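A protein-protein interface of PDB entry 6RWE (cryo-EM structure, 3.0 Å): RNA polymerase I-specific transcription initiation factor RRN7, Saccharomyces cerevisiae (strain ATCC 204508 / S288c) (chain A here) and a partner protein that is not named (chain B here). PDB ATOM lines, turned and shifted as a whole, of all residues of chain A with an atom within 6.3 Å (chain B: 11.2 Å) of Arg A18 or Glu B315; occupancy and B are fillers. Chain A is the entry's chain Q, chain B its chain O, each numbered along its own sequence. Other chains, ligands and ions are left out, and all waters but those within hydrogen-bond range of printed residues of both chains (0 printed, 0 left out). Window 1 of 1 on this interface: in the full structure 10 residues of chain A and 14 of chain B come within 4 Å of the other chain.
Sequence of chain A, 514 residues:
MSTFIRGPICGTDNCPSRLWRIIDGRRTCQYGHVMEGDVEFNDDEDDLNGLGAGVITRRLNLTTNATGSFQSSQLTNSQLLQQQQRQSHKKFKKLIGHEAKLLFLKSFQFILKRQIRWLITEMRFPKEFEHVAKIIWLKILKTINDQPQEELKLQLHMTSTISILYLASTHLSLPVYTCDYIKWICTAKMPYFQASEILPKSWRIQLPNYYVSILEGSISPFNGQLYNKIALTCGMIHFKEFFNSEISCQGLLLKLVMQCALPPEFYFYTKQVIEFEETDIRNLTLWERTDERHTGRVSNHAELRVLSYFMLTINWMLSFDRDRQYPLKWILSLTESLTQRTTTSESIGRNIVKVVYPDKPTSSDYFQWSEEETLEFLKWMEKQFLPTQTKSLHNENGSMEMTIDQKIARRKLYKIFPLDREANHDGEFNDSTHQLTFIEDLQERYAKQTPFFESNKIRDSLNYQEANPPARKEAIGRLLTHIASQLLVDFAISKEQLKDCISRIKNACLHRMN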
ATOM      1  N   THR A   3      29.448  11.231 -10.736  1.00  0.00           N
ATOM      2  CA  THR A   3      30.143  10.167 -10.028  1.00  0.00           C
ATOM      3  C   THR A   3      30.439   8.974 -10.934  1.00  0.00           C
ATOM      4  O   THR A   3      31.407   8.249 -10.723  1.00  0.00           O
ATOM      5  CB  THR A   3      29.328   9.689  -8.812  1.00  0.00           C
ATOM      6  OG1 THR A   3      28.027   9.269  -9.243  1.00  0.00           O
ATOM      7  CG2 THR A   3      29.184  10.801  -7.787  1.00  0.00           C
ATOM      8  N   PHE A   4      29.600   8.791 -11.947  1.00  0.00           N
ATOM      9  CA  PHE A   4      29.640   7.633 -12.825  1.00  0.00           C
ATOM     10  C   PHE A   4      30.707   7.806 -13.902  1.00  0.00           C
ATOM     11  O   PHE A   4      31.280   8.882 -14.083  1.00  0.00           O
ATOM     12  CB  PHE A   4      28.277   7.429 -13.472  1.00  0.00           C
ATOM     13  CG  PHE A   4      27.201   7.053 -12.508  1.00  0.00           C
ATOM     14  CD1 PHE A   4      26.975   5.730 -12.195  1.00  0.00           C
ATOM     15  CD2 PHE A   4      26.430   8.023 -11.897  1.00  0.00           C
ATOM     16  CE1 PHE A   4      25.992   5.375 -11.298  1.00  0.00           C
ATOM     17  CE2 PHE A   4      25.449   7.673 -10.996  1.00  0.00           C
ATOM     18  CZ  PHE A   4      25.228   6.349 -10.699  1.00  0.00           C
ATOM     19  N   ILE A   5      30.975   6.718 -14.625  1.00  0.00           N
ATOM     20  CA  ILE A   5      31.804   6.755 -15.824  1.00  0.00           C
ATOM     21  C   ILE A   5      31.065   6.041 -16.944  1.00  0.00           C
ATOM     22  O   ILE A   5      30.276   5.123 -16.709  1.00  0.00           O
ATOM     23  CB  ILE A   5      33.207   6.131 -15.618  1.00  0.00           C
ATOM     24  CG1 ILE A   5      33.106   4.678 -15.165  1.00  0.00           C
ATOM     25  CG2 ILE A   5      34.031   6.943 -14.638  1.00  0.00           C
ATOM     26  CD1 ILE A   5      34.420   3.940 -15.182  1.00  0.00           C
ATOM     27  N   ARG A   6      31.309   6.486 -18.169  1.00  0.00           N
ATOM     28  CA  ARG A   6      30.682   5.876 -19.332  1.00  0.00           C
ATOM     29  C   ARG A   6      31.269   4.494 -19.581  1.00  0.00           C
ATOM     30  O   ARG A   6      32.480   4.291 -19.487  1.00  0.00           O
ATOM     31  CB  ARG A   6      30.881   6.766 -20.556  1.00  0.00           C
ATOM     32  CG  ARG A   6      30.290   6.239 -21.851  1.00  0.00           C
ATOM     33  CD  ARG A   6      28.779   6.304 -21.865  1.00  0.00           C
ATOM     34  NE  ARG A   6      28.237   5.823 -23.132  1.00  0.00           N
ATOM     35  CZ  ARG A   6      26.940   5.702 -23.396  1.00  0.00           C
ATOM     36  NH1 ARG A   6      26.038   6.046 -22.487  1.00  0.00           N
ATOM     37  NH2 ARG A   6      26.546   5.249 -24.578  1.00  0.00           N
ATOM     38  N   GLY A   7      30.404   3.537 -19.889  1.00  0.00           N
ATOM     39  CA  GLY A   7      30.849   2.196 -20.167  1.00  0.00           C
ATOM     40  C   GLY A   7      29.942   1.481 -21.142  1.00  0.00           C
ATOM     41  O   GLY A   7      29.135   2.100 -21.839  1.00  0.00           O
ATOM     42  N   PRO A   8      30.056   0.158 -21.212  1.00  0.00           N
ATOM     43  CA  PRO A   8      29.174  -0.612 -22.091  1.00  0.00           C
ATOM     44  C   PRO A   8      27.782  -0.736 -21.500  1.00  0.00           C
ATOM     45  O   PRO A   8      27.508  -0.325 -20.374  1.00  0.00           O
ATOM     46  CB  PRO A   8      29.863  -1.971 -22.173  1.00  0.00           C
ATOM     47  CG  PRO A   8      30.585  -2.080 -20.897  1.00  0.00           C
ATOM     48  CD  PRO A   8      31.048  -0.701 -20.550  1.00  0.00           C
ATOM     49  N   CYS A  15      19.510  -1.448 -19.426  1.00  0.00           N
ATOM     50  CA  CYS A  15      19.274  -0.260 -20.238  1.00  0.00           C
ATOM     51  C   CYS A  15      20.621   0.081 -20.852  1.00  0.00           C
ATOM     52  O   CYS A  15      21.631  -0.502 -20.438  1.00  0.00           O
ATOM     53  CB  CYS A  15      18.744   0.917 -19.418  1.00  0.00           C
ATOM     54  SG  CYS A  15      19.896   1.547 -18.214  1.00  0.00           S
ATOM     55  N   PRO A  16      20.702   0.992 -21.840  1.00  0.00           N
ATOM     56  CA  PRO A  16      22.011   1.585 -22.147  1.00  0.00           C
ATOM     57  C   PRO A  16      22.511   2.390 -20.959  1.00  0.00           C
ATOM     58  O   PRO A  16      21.976   3.459 -20.649  1.00  0.00           O
ATOM     59  CB  PRO A  16      21.726   2.472 -23.365  1.00  0.00           C
ATOM     60  CG  PRO A  16      20.535   1.853 -24.000  1.00  0.00           C
ATOM     61  CD  PRO A  16      19.701   1.329 -22.870  1.00  0.00           C
ATOM     62  N   SER A  17      23.539   1.883 -20.288  1.00  0.00           N
ATOM     63  CA  SER A  17      23.907   2.375 -18.973  1.00  0.00           C
ATOM     64  C   SER A  17      25.350   2.847 -18.962  1.00  0.00           C
ATOM     65  O   SER A  17      26.126   2.616 -19.893  1.00  0.00           O
ATOM     66  CB  SER A  17      23.714   1.302 -17.897  1.00  0.00           C
ATOM     67  OG  SER A  17      22.355   0.975 -17.736  1.00  0.00           O
ATOM     68  N   ARG A  18      25.683   3.514 -17.869  1.00  0.00           N
ATOM     69  CA  ARG A  18      27.027   3.954 -17.559  1.00  0.00           C
ATOM     70  C   ARG A  18      27.350   3.442 -16.163  1.00  0.00           C
ATOM     71  O   ARG A  18      26.465   3.348 -15.309  1.00  0.00           O
ATOM     72  CB  ARG A  18      27.158   5.491 -17.677  1.00  0.00           C
ATOM     73  CG  ARG A  18      26.630   6.343 -16.530  1.00  0.00           C
ATOM     74  CD  ARG A  18      25.123   6.461 -16.515  1.00  0.00           C
ATOM     75  NE  ARG A  18      24.621   7.072 -17.736  1.00  0.00           N
ATOM     76  CZ  ARG A  18      23.420   6.826 -18.253  1.00  0.00           C
ATOM     77  NH1 ARG A  18      23.041   7.425 -19.376  1.00  0.00           N
ATOM     78  NH2 ARG A  18      22.599   5.978 -17.646  1.00  0.00           N
ATOM     79  N   LEU A  19      28.603   3.065 -15.949  1.00  0.00           N
ATOM     80  CA  LEU A  19      28.968   2.231 -14.816  1.00  0.00           C
ATOM     81  C   LEU A  19      29.752   3.034 -13.784  1.00  0.00           C
ATOM     82  O   LEU A  19      30.057   4.212 -13.976  1.00  0.00           O
ATOM     83  CB  LEU A  19      29.738   0.993 -15.285  1.00  0.00           C
ATOM     84  CG  LEU A  19      28.867  -0.160 -15.816  1.00  0.00           C
ATOM     85  CD1 LEU A  19      28.428   0.026 -17.244  1.00  0.00           C
ATOM     86  CD2 LEU A  19      29.515  -1.513 -15.641  1.00  0.00           C
ATOM     87  N   TRP A  20      30.065   2.379 -12.665  1.00  0.00           N
ATOM     88  CA  TRP A  20      30.669   3.046 -11.512  1.00  0.00           C
ATOM     89  C   TRP A  20      31.265   1.999 -10.590  1.00  0.00           C
ATOM     90  O   TRP A  20      30.542   1.114 -10.127  1.00  0.00           O
ATOM     91  CB  TRP A  20      29.623   3.875 -10.783  1.00  0.00           C
ATOM     92  CG  TRP A  20      30.098   4.597  -9.587  1.00  0.00           C
ATOM     93  CD1 TRP A  20      31.216   5.367  -9.488  1.00  0.00           C
ATOM     94  CD2 TRP A  20      29.404   4.737  -8.345  1.00  0.00           C
ATOM     95  NE1 TRP A  20      31.300   5.925  -8.236  1.00  0.00           N
ATOM     96  CE2 TRP A  20      30.194   5.558  -7.515  1.00  0.00           C
ATOM     97  CE3 TRP A  20      28.204   4.227  -7.841  1.00  0.00           C
ATOM     98  CZ2 TRP A  20      29.828   5.876  -6.209  1.00  0.00           C
ATOM     99  CZ3 TRP A  20      27.836   4.546  -6.544  1.00  0.00           C
ATOM    100  CH2 TRP A  20      28.648   5.360  -5.742  1.00  0.00           C
ATOM    101  N   THR A  28      29.383  -1.557 -10.731  1.00  0.00           N
ATOM    102  CA  THR A  28      27.951  -1.726 -10.886  1.00  0.00           C
ATOM    103  C   THR A  28      27.439  -0.863 -12.023  1.00  0.00           C
ATOM    104  O   THR A  28      28.144  -0.011 -12.551  1.00  0.00           O
ATOM    105  CB  THR A  28      27.208  -1.348  -9.616  1.00  0.00           C
ATOM    106  OG1 THR A  28      27.493   0.016  -9.292  1.00  0.00           O
ATOM    107  CG2 THR A  28      27.628  -2.218  -8.501  1.00  0.00           C
ATOM    108  N   CYS A  29      26.180  -1.075 -12.379  1.00  0.00           N
ATOM    109  CA  CYS A  29      25.514  -0.185 -13.315  1.00  0.00           C
ATOM    110  C   CYS A  29      24.931   0.983 -12.530  1.00  0.00           C
ATOM    111  O   CYS A  29      25.246   1.201 -11.358  1.00  0.00           O
ATOM    112  CB  CYS A  29      24.445  -0.925 -14.109  1.00  0.00           C
ATOM    113  SG  CYS A  29      22.994  -1.381 -13.167  1.00  0.00           S
ATOM    114  N   GLN A  30      24.080   1.763 -13.186  1.00  0.00           N
ATOM    115  CA  GLN A  30      23.364   2.832 -12.505  1.00  0.00           C
ATOM    116  C   GLN A  30      22.369   2.282 -11.495  1.00  0.00           C
ATOM    117  O   GLN A  30      22.154   2.884 -10.438  1.00  0.00           O
ATOM    118  CB  GLN A  30      22.655   3.692 -13.543  1.00  0.00           C
ATOM    119  CG  GLN A  30      21.853   4.835 -12.995  1.00  0.00           C
ATOM    120  CD  GLN A  30      21.208   5.639 -14.088  1.00  0.00           C
ATOM    121  OE1 GLN A  30      21.401   5.362 -15.271  1.00  0.00           O
ATOM    122  NE2 GLN A  30      20.413   6.629 -13.703  1.00  0.00           N
ATOM    123  N   TYR A  31      21.787   1.125 -11.783  1.00  0.00           N
ATOM    124  CA  TYR A  31      20.671   0.596 -11.018  1.00  0.00           C
ATOM    125  C   TYR A  31      21.109  -0.460 -10.016  1.00  0.00           C
ATOM    126  O   TYR A  31      20.259  -1.091  -9.387  1.00  0.00           O
ATOM    127  CB  TYR A  31      19.629   0.025 -11.978  1.00  0.00           C
ATOM    128  CG  TYR A  31      19.043   1.058 -12.920  1.00  0.00           C
ATOM    129  CD1 TYR A  31      18.958   2.397 -12.563  1.00  0.00           C
ATOM    130  CD2 TYR A  31      18.657   0.703 -14.201  1.00  0.00           C
ATOM    131  CE1 TYR A  31      18.452   3.338 -13.440  1.00  0.00           C
ATOM    132  CE2 TYR A  31      18.159   1.632 -15.081  1.00  0.00           C
ATOM    133  CZ  TYR A  31      18.056   2.944 -14.697  1.00  0.00           C
ATOM    134  OH  TYR A  31      17.556   3.866 -15.581  1.00  0.00           O
ATOM    135  N   ASN B 200      13.226  -4.683 -19.645  1.00  0.00           N
ATOM    136  CA  ASN B 200      13.548  -4.463 -18.249  1.00  0.00           C
ATOM    137  C   ASN B 200      12.278  -4.166 -17.461  1.00  0.00           C
ATOM    138  O   ASN B 200      11.184  -4.035 -18.011  1.00  0.00           O
ATOM    139  CB  ASN B 200      14.523  -3.299 -18.097  1.00  0.00           C
ATOM    140  CG  ASN B 200      15.374  -3.412 -16.845  1.00  0.00           C
ATOM    141  OD1 ASN B 200      15.276  -4.391 -16.107  1.00  0.00           O
ATOM    142  ND2 ASN B 200      16.199  -2.408 -16.592  1.00  0.00           N
ATOM    143  N   ASN B 202      12.452  -1.268 -16.079  1.00  0.00           N
ATOM    144  CA  ASN B 202      12.413   0.160 -16.356  1.00  0.00           C
ATOM    145  C   ASN B 202      12.941   0.528 -17.741  1.00  0.00           C
ATOM    146  O   ASN B 202      13.763   1.440 -17.875  1.00  0.00           O
ATOM    147  CB  ASN B 202      13.153   0.920 -15.252  1.00  0.00           C
ATOM    148  CG  ASN B 202      14.562   0.418 -15.023  1.00  0.00           C
ATOM    149  OD1 ASN B 202      15.075  -0.406 -15.772  1.00  0.00           O
ATOM    150  ND2 ASN B 202      15.183   0.903 -13.961  1.00  0.00           N
ATOM    151  N   ASP B 203      12.482  -0.184 -18.771  1.00  0.00           N
ATOM    152  CA  ASP B 203      12.550   0.296 -20.144  1.00  0.00           C
ATOM    153  C   ASP B 203      11.323   1.159 -20.430  1.00  0.00           C
ATOM    154  O   ASP B 203      10.563   1.507 -19.526  1.00  0.00           O
ATOM    155  CB  ASP B 203      12.635  -0.863 -21.135  1.00  0.00           C
ATOM    156  CG  ASP B 203      14.004  -1.474 -21.197  1.00  0.00           C
ATOM    157  OD1 ASP B 203      14.989  -0.747 -20.974  1.00  0.00           O
ATOM    158  OD2 ASP B 203      14.094  -2.686 -21.480  1.00  0.00           O
ATOM    159  N   GLU B 309      31.740   6.391 -31.285  1.00  0.00           N
ATOM    160  CA  GLU B 309      33.014   6.967 -30.884  1.00  0.00           C
ATOM    161  C   GLU B 309      33.617   6.140 -29.752  1.00  0.00           C
ATOM    162  O   GLU B 309      33.094   5.093 -29.362  1.00  0.00           O
ATOM    163  CB  GLU B 309      32.844   8.427 -30.463  1.00  0.00           C
ATOM    164  CG  GLU B 309      32.486   9.369 -31.592  1.00  0.00           C
ATOM    165  CD  GLU B 309      32.348  10.800 -31.121  1.00  0.00           C
ATOM    166  OE1 GLU B 309      32.411  11.026 -29.895  1.00  0.00           O
ATOM    167  OE2 GLU B 309      32.178  11.698 -31.972  1.00  0.00           O
ATOM    168  N   GLY B 310      34.737   6.625 -29.223  1.00  0.00           N
ATOM    169  CA  GLY B 310      35.397   5.963 -28.115  1.00  0.00           C
ATOM    170  C   GLY B 310      34.876   6.418 -26.769  1.00  0.00           C
ATOM    171  O   GLY B 310      35.570   7.126 -26.036  1.00  0.00           O
ATOM    172  N   MET B 311      33.654   6.010 -26.430  1.00  0.00           N
ATOM    173  CA  MET B 311      32.981   6.465 -25.215  1.00  0.00           C
ATOM    174  C   MET B 311      33.423   5.599 -24.042  1.00  0.00           C
ATOM    175  O   MET B 311      32.826   4.566 -23.743  1.00  0.00           O
ATOM    176  CB  MET B 311      31.468   6.432 -25.394  1.00  0.00           C
ATOM    177  CG  MET B 311      30.934   7.456 -26.378  1.00  0.00           C
ATOM    178  SD  MET B 311      31.307   9.138 -25.858  1.00  0.00           S
ATOM    179  CE  MET B 311      30.274   9.272 -24.404  1.00  0.00           C
ATOM    180  N   ASP B 312      34.479   6.044 -23.359  1.00  0.00           N
ATOM    181  CA  ASP B 312      34.971   5.387 -22.158  1.00  0.00           C
ATOM    182  C   ASP B 312      35.198   6.352 -21.002  1.00  0.00           C
ATOM    183  O   ASP B 312      35.616   5.912 -19.928  1.00  0.00           O
ATOM    184  CB  ASP B 312      36.285   4.642 -22.444  1.00  0.00           C
ATOM    185  CG  ASP B 312      36.084   3.412 -23.300  1.00  0.00           C
ATOM    186  OD1 ASP B 312      35.008   2.789 -23.209  1.00  0.00           O
ATOM    187  OD2 ASP B 312      37.007   3.064 -24.067  1.00  0.00           O
ATOM    188  N   GLY B 313      34.943   7.643 -21.189  1.00  0.00           N
ATOM    189  CA  GLY B 313      35.223   8.622 -20.158  1.00  0.00           C
ATOM    190  C   GLY B 313      34.122   8.749 -19.129  1.00  0.00           C
ATOM    191  O   GLY B 313      33.590   7.743 -18.656  1.00  0.00           O
ATOM    192  N   THR B 314      33.767   9.979 -18.777  1.00  0.00           N
ATOM    193  CA  THR B 314      32.773  10.232 -17.750  1.00  0.00           C
ATOM    194  C   THR B 314      31.528  10.863 -18.350  1.00  0.00           C
ATOM    195  O   THR B 314      31.594  11.617 -19.326  1.00  0.00           O
ATOM    196  CB  THR B 314      33.318  11.153 -16.654  1.00  0.00           C
ATOM    197  OG1 THR B 314      33.667  12.418 -17.227  1.00  0.00           O
ATOM    198  CG2 THR B 314      34.545  10.551 -16.008  1.00  0.00           C
ATOM    199  N   GLU B 315      30.387  10.523 -17.761  1.00  0.00           N
ATOM    200  CA  GLU B 315      29.130  11.242 -17.910  1.00  0.00           C
ATOM    201  C   GLU B 315      28.602  11.573 -16.529  1.00  0.00           C
ATOM    202  O   GLU B 315      27.441  11.343 -16.186  1.00  0.00           O
ATOM    203  CB  GLU B 315      28.120  10.448 -18.731  1.00  0.00           C
ATOM    204  CG  GLU B 315      28.527  10.285 -20.190  1.00  0.00           C
ATOM    205  CD  GLU B 315      27.515   9.510 -21.006  1.00  0.00           C
ATOM    206  OE1 GLU B 315      26.537   8.998 -20.425  1.00  0.00           O
ATOM    207  OE2 GLU B 315      27.703   9.412 -22.235  1.00  0.00           O
ATOM    208  N   GLU B 316      29.500  12.111 -15.714  1.00  0.00           N
ATOM    209  CA  GLU B 316      29.296  12.300 -14.290  1.00  0.00           C
ATOM    210  C   GLU B 316      28.307  13.420 -13.999  1.00  0.00           C
ATOM    211  O   GLU B 316      28.100  14.333 -14.804  1.00  0.00           O
ATOM    212  CB  GLU B 316      30.631  12.605 -13.619  1.00  0.00           C
ATOM    213  CG  GLU B 316      31.344  13.811 -14.201  1.00  0.00           C
ATOM    214  CD  GLU B 316      32.721  13.996 -13.605  1.00  0.00           C
ATOM    215  OE1 GLU B 316      33.060  13.255 -12.662  1.00  0.00           O
ATOM    216  OE2 GLU B 316      33.483  14.843 -14.110  1.00  0.00           O
ATOM    217  N   TYR B 317      27.679  13.313 -12.825  1.00  0.00           N
ATOM    218  CA  TYR B 317      26.794  14.315 -12.223  1.00  0.00           C
ATOM    219  C   TYR B 317      25.586  14.646 -13.095  1.00  0.00           C
ATOM    220  O   TYR B 317      25.004  15.728 -12.977  1.00  0.00           O
ATOM    221  CB  TYR B 317      27.569  15.586 -11.861  1.00  0.00           C
ATOM    222  CG  TYR B 317      28.587  15.366 -10.762  1.00  0.00           C
ATOM    223  CD1 TYR B 317      28.205  15.340  -9.426  1.00  0.00           C
ATOM    224  CD2 TYR B 317      29.931  15.175 -11.063  1.00  0.00           C
ATOM    225  CE1 TYR B 317      29.133  15.140  -8.420  1.00  0.00           C
ATOM    226  CE2 TYR B 317      30.867  14.971 -10.063  1.00  0.00           C
ATOM    227  CZ  TYR B 317      30.464  14.956  -8.746  1.00  0.00           C
ATOM    228  OH  TYR B 317      31.399  14.753  -7.755  1.00  0.00           O
ATOM    229  N   ASN B 318      25.200  13.712 -13.956  1.00  0.00           N
ATOM    230  CA  ASN B 318      23.998  13.770 -14.775  1.00  0.00           C
ATOM    231  C   ASN B 318      23.176  12.523 -14.516  1.00  0.00           C
ATOM    232  O   ASN B 318      22.742  11.813 -15.425  1.00  0.00           O
ATOM    233  CB  ASN B 318      24.348  13.928 -16.250  1.00  0.00           C
ATOM    234  CG  ASN B 318      24.927  15.295 -16.565  1.00  0.00           C
ATOM    235  OD1 ASN B 318      24.457  16.315 -16.060  1.00  0.00           O
ATOM    236  ND2 ASN B 318      25.956  15.323 -17.403  1.00  0.00           N
ATOM    237  N   VAL B 319      22.976  12.256 -13.225  1.00  0.00           N
ATOM    238  CA  VAL B 319      22.542  10.944 -12.760  1.00  0.00           C
ATOM    239  C   VAL B 319      21.075  10.706 -13.091  1.00  0.00           C
ATOM    240  O   VAL B 319      20.705   9.629 -13.574  1.00  0.00           O
ATOM    241  CB  VAL B 319      22.801  10.829 -11.249  1.00  0.00           C
ATOM    242  CG1 VAL B 319      22.353   9.482 -10.722  1.00  0.00           C
ATOM    243  CG2 VAL B 319      24.268  11.101 -10.944  1.00  0.00           C
ATOM    244  N   GLU B 320      20.226  11.707 -12.814  1.00  0.00           N
ATOM    245  CA  GLU B 320      18.759  11.731 -12.904  1.00  0.00           C
ATOM    246  C   GLU B 320      18.077  10.481 -12.347  1.00  0.00           C
ATOM    247  O   GLU B 320      17.004  10.086 -12.815  1.00  0.00           O
ATOM    248  CB  GLU B 320      18.286  12.029 -14.347  1.00  0.00           C
ATOM    249  CG  GLU B 320      18.552  11.007 -15.465  1.00  0.00           C
ATOM    250  CD  GLU B 320      18.104  11.495 -16.828  1.00  0.00           C
ATOM    251  OE1 GLU B 320      17.618  12.641 -16.921  1.00  0.00           O
ATOM    252  OE2 GLU B 320      18.237  10.733 -17.807  1.00  0.00           O
ATOM    253  N   LEU B 321      18.658   9.883 -11.306  1.00  0.00           N
ATOM    254  CA  LEU B 321      18.065   8.711 -10.666  1.00  0.00           C
ATOM    255  C   LEU B 321      16.982   9.229  -9.728  1.00  0.00           C
ATOM    256  O   LEU B 321      17.189   9.450  -8.533  1.00  0.00           O
ATOM    257  CB  LEU B 321      19.123   7.886  -9.939  1.00  0.00           C
ATOM    258  CG  LEU B 321      18.844   6.430  -9.542  1.00  0.00           C
ATOM    259  CD1 LEU B 321      20.146   5.667  -9.526  1.00  0.00           C
ATOM    260  CD2 LEU B 321      18.159   6.294  -8.192  1.00  0.00           C
ATOM    261  N   THR B 322      15.809   9.467 -10.308  1.00  0.00           N
ATOM    262  CA  THR B 322      14.617   9.874  -9.564  1.00  0.00           C
ATOM    263  C   THR B 322      13.460   9.148 -10.245  1.00  0.00           C
ATOM    264  O   THR B 322      12.903   9.629 -11.236  1.00  0.00           O
ATOM    265  CB  THR B 322      14.431  11.388  -9.560  1.00  0.00           C
ATOM    266  OG1 THR B 322      15.600  12.012  -9.014  1.00  0.00           O
ATOM    267  CG2 THR B 322      13.227  11.775  -8.712  1.00  0.00           C
ATOM    268  N   GLN B 323      13.120   7.975  -9.720  1.00  0.00           N
ATOM    269  CA  GLN B 323      12.148   7.112 -10.371  1.00  0.00           C
ATOM    270  C   GLN B 323      10.741   7.638 -10.125  1.00  0.00           C
ATOM    271  O   GLN B 323      10.386   8.008  -9.003  1.00  0.00           O
ATOM    272  CB  GLN B 323      12.288   5.679  -9.863  1.00  0.00           C
ATOM    273  CG  GLN B 323      11.491   4.676 -10.658  1.00  0.00           C
ATOM    274  CD  GLN B 323      11.939   4.600 -12.106  1.00  0.00           C
ATOM    275  OE1 GLN B 323      11.281   5.128 -12.999  1.00  0.00           O
ATOM    276  NE2 GLN B 323      13.061   3.936 -12.346  1.00  0.00           N
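Glu B316 touches Thr A3.
O of Phe A4 touches CB of Thr B314 (3.99 Å).
Glu B316 touches Phe A4 (CB to O, 3.8 Å).
Val B319 touches Phe A4 (CG1 to CE2, 3.6 Å).
Gly B313 touches Ile A5.
Thr B314 touches Ile A5.
Arg A6 touches Met B311.
Arg A6 touches Asp B312.
Leu B321 touches Gln A30.
ND2 of Asn B202 touches CE2 of Tyr A31 (3.3 Å).
The backbone NH (N) of Arg A6 sits at hydrogen-bond distance from the backbone carbonyl oxygen (O) of Gly B313 (2.6 Å).
The backbone NH (N) of Tyr B317 lies close to the backbone NH (N) of Thr A3 (3.4 Å).
NE of Arg A18 lies within salt-bridge range of OE1 of Glu B315 (3.8 Å).
NE2 of Gln A30 lies within hydrogen-bond range of O of Val B319 (3.0 Å).
The side-chain carboxylate (OE1) of Glu B315 is in salt-bridge range of the guanidinium group (NH1) of Arg A6 (3.6 Å).
Arg A6 touches four residues of chain B.
No residue of chain B comes within 4 Å of Ser A17.
Of chain B, only Glu B315 comes within 4 Å of Arg A18.
Asp B203 touches none of the printed residues of chain A.
Printed residues of chain A within 4 Å of Met B311: Arg A6 (3.6 Å).
Of the printed residues of chain A, Asp B312 touches Arg A6 (3.6 Å).
Of the printed residues of chain A, Gly B313 touches Ile A5 and Arg A6.
Glu B315 touches just these residues of chain A: Arg A6 (3.3 Å) and Arg A18 (3.8 Å).
Printed residues of chain A within 4 Å of Tyr B317: Thr A3 (3.4 Å).
The nearest residue of chain B that does not touch Arg A18 is Asn B318 (5.6 Å).
Hydrophobic or aromatic side chains of chain B that line the printed part of chain A: Met B311, Tyr B317, Val B319 and Leu B321.
Of the 16 printed residues of chain A, 7 touch a printed residue of chain B.
Among the printed residues, 15 pairs touch across the chains.
Among the printed residues, Asp or Glu carboxylates within 4 Å of a Lys or Arg side-chain nitrogen of the other chain: Arg A6 with Glu B315 (3.6 Å) and Arg A18 with Glu B315 (3.8 Å).
The side-chain amide oxygen (OE1) of Gln A30 is in hydrogen-bond range of the guanidinium group (NH2) of Arg A18, at 2.7 Å.
ND2 of Asn B200 is in hydrogen-bond range of OD1 of Asn B202, 2.4 Å away.
The backbone NH (N) of Tyr A31 sits close to the side-chain sulfur (SG) of Cys A29, 3.1 Å away.
O of Leu A19 is in hydrogen-bond range of N of Ile A5.
The backbone carbonyl oxygen of Thr A3 lies close to the indole nitrogen of Trp A20.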
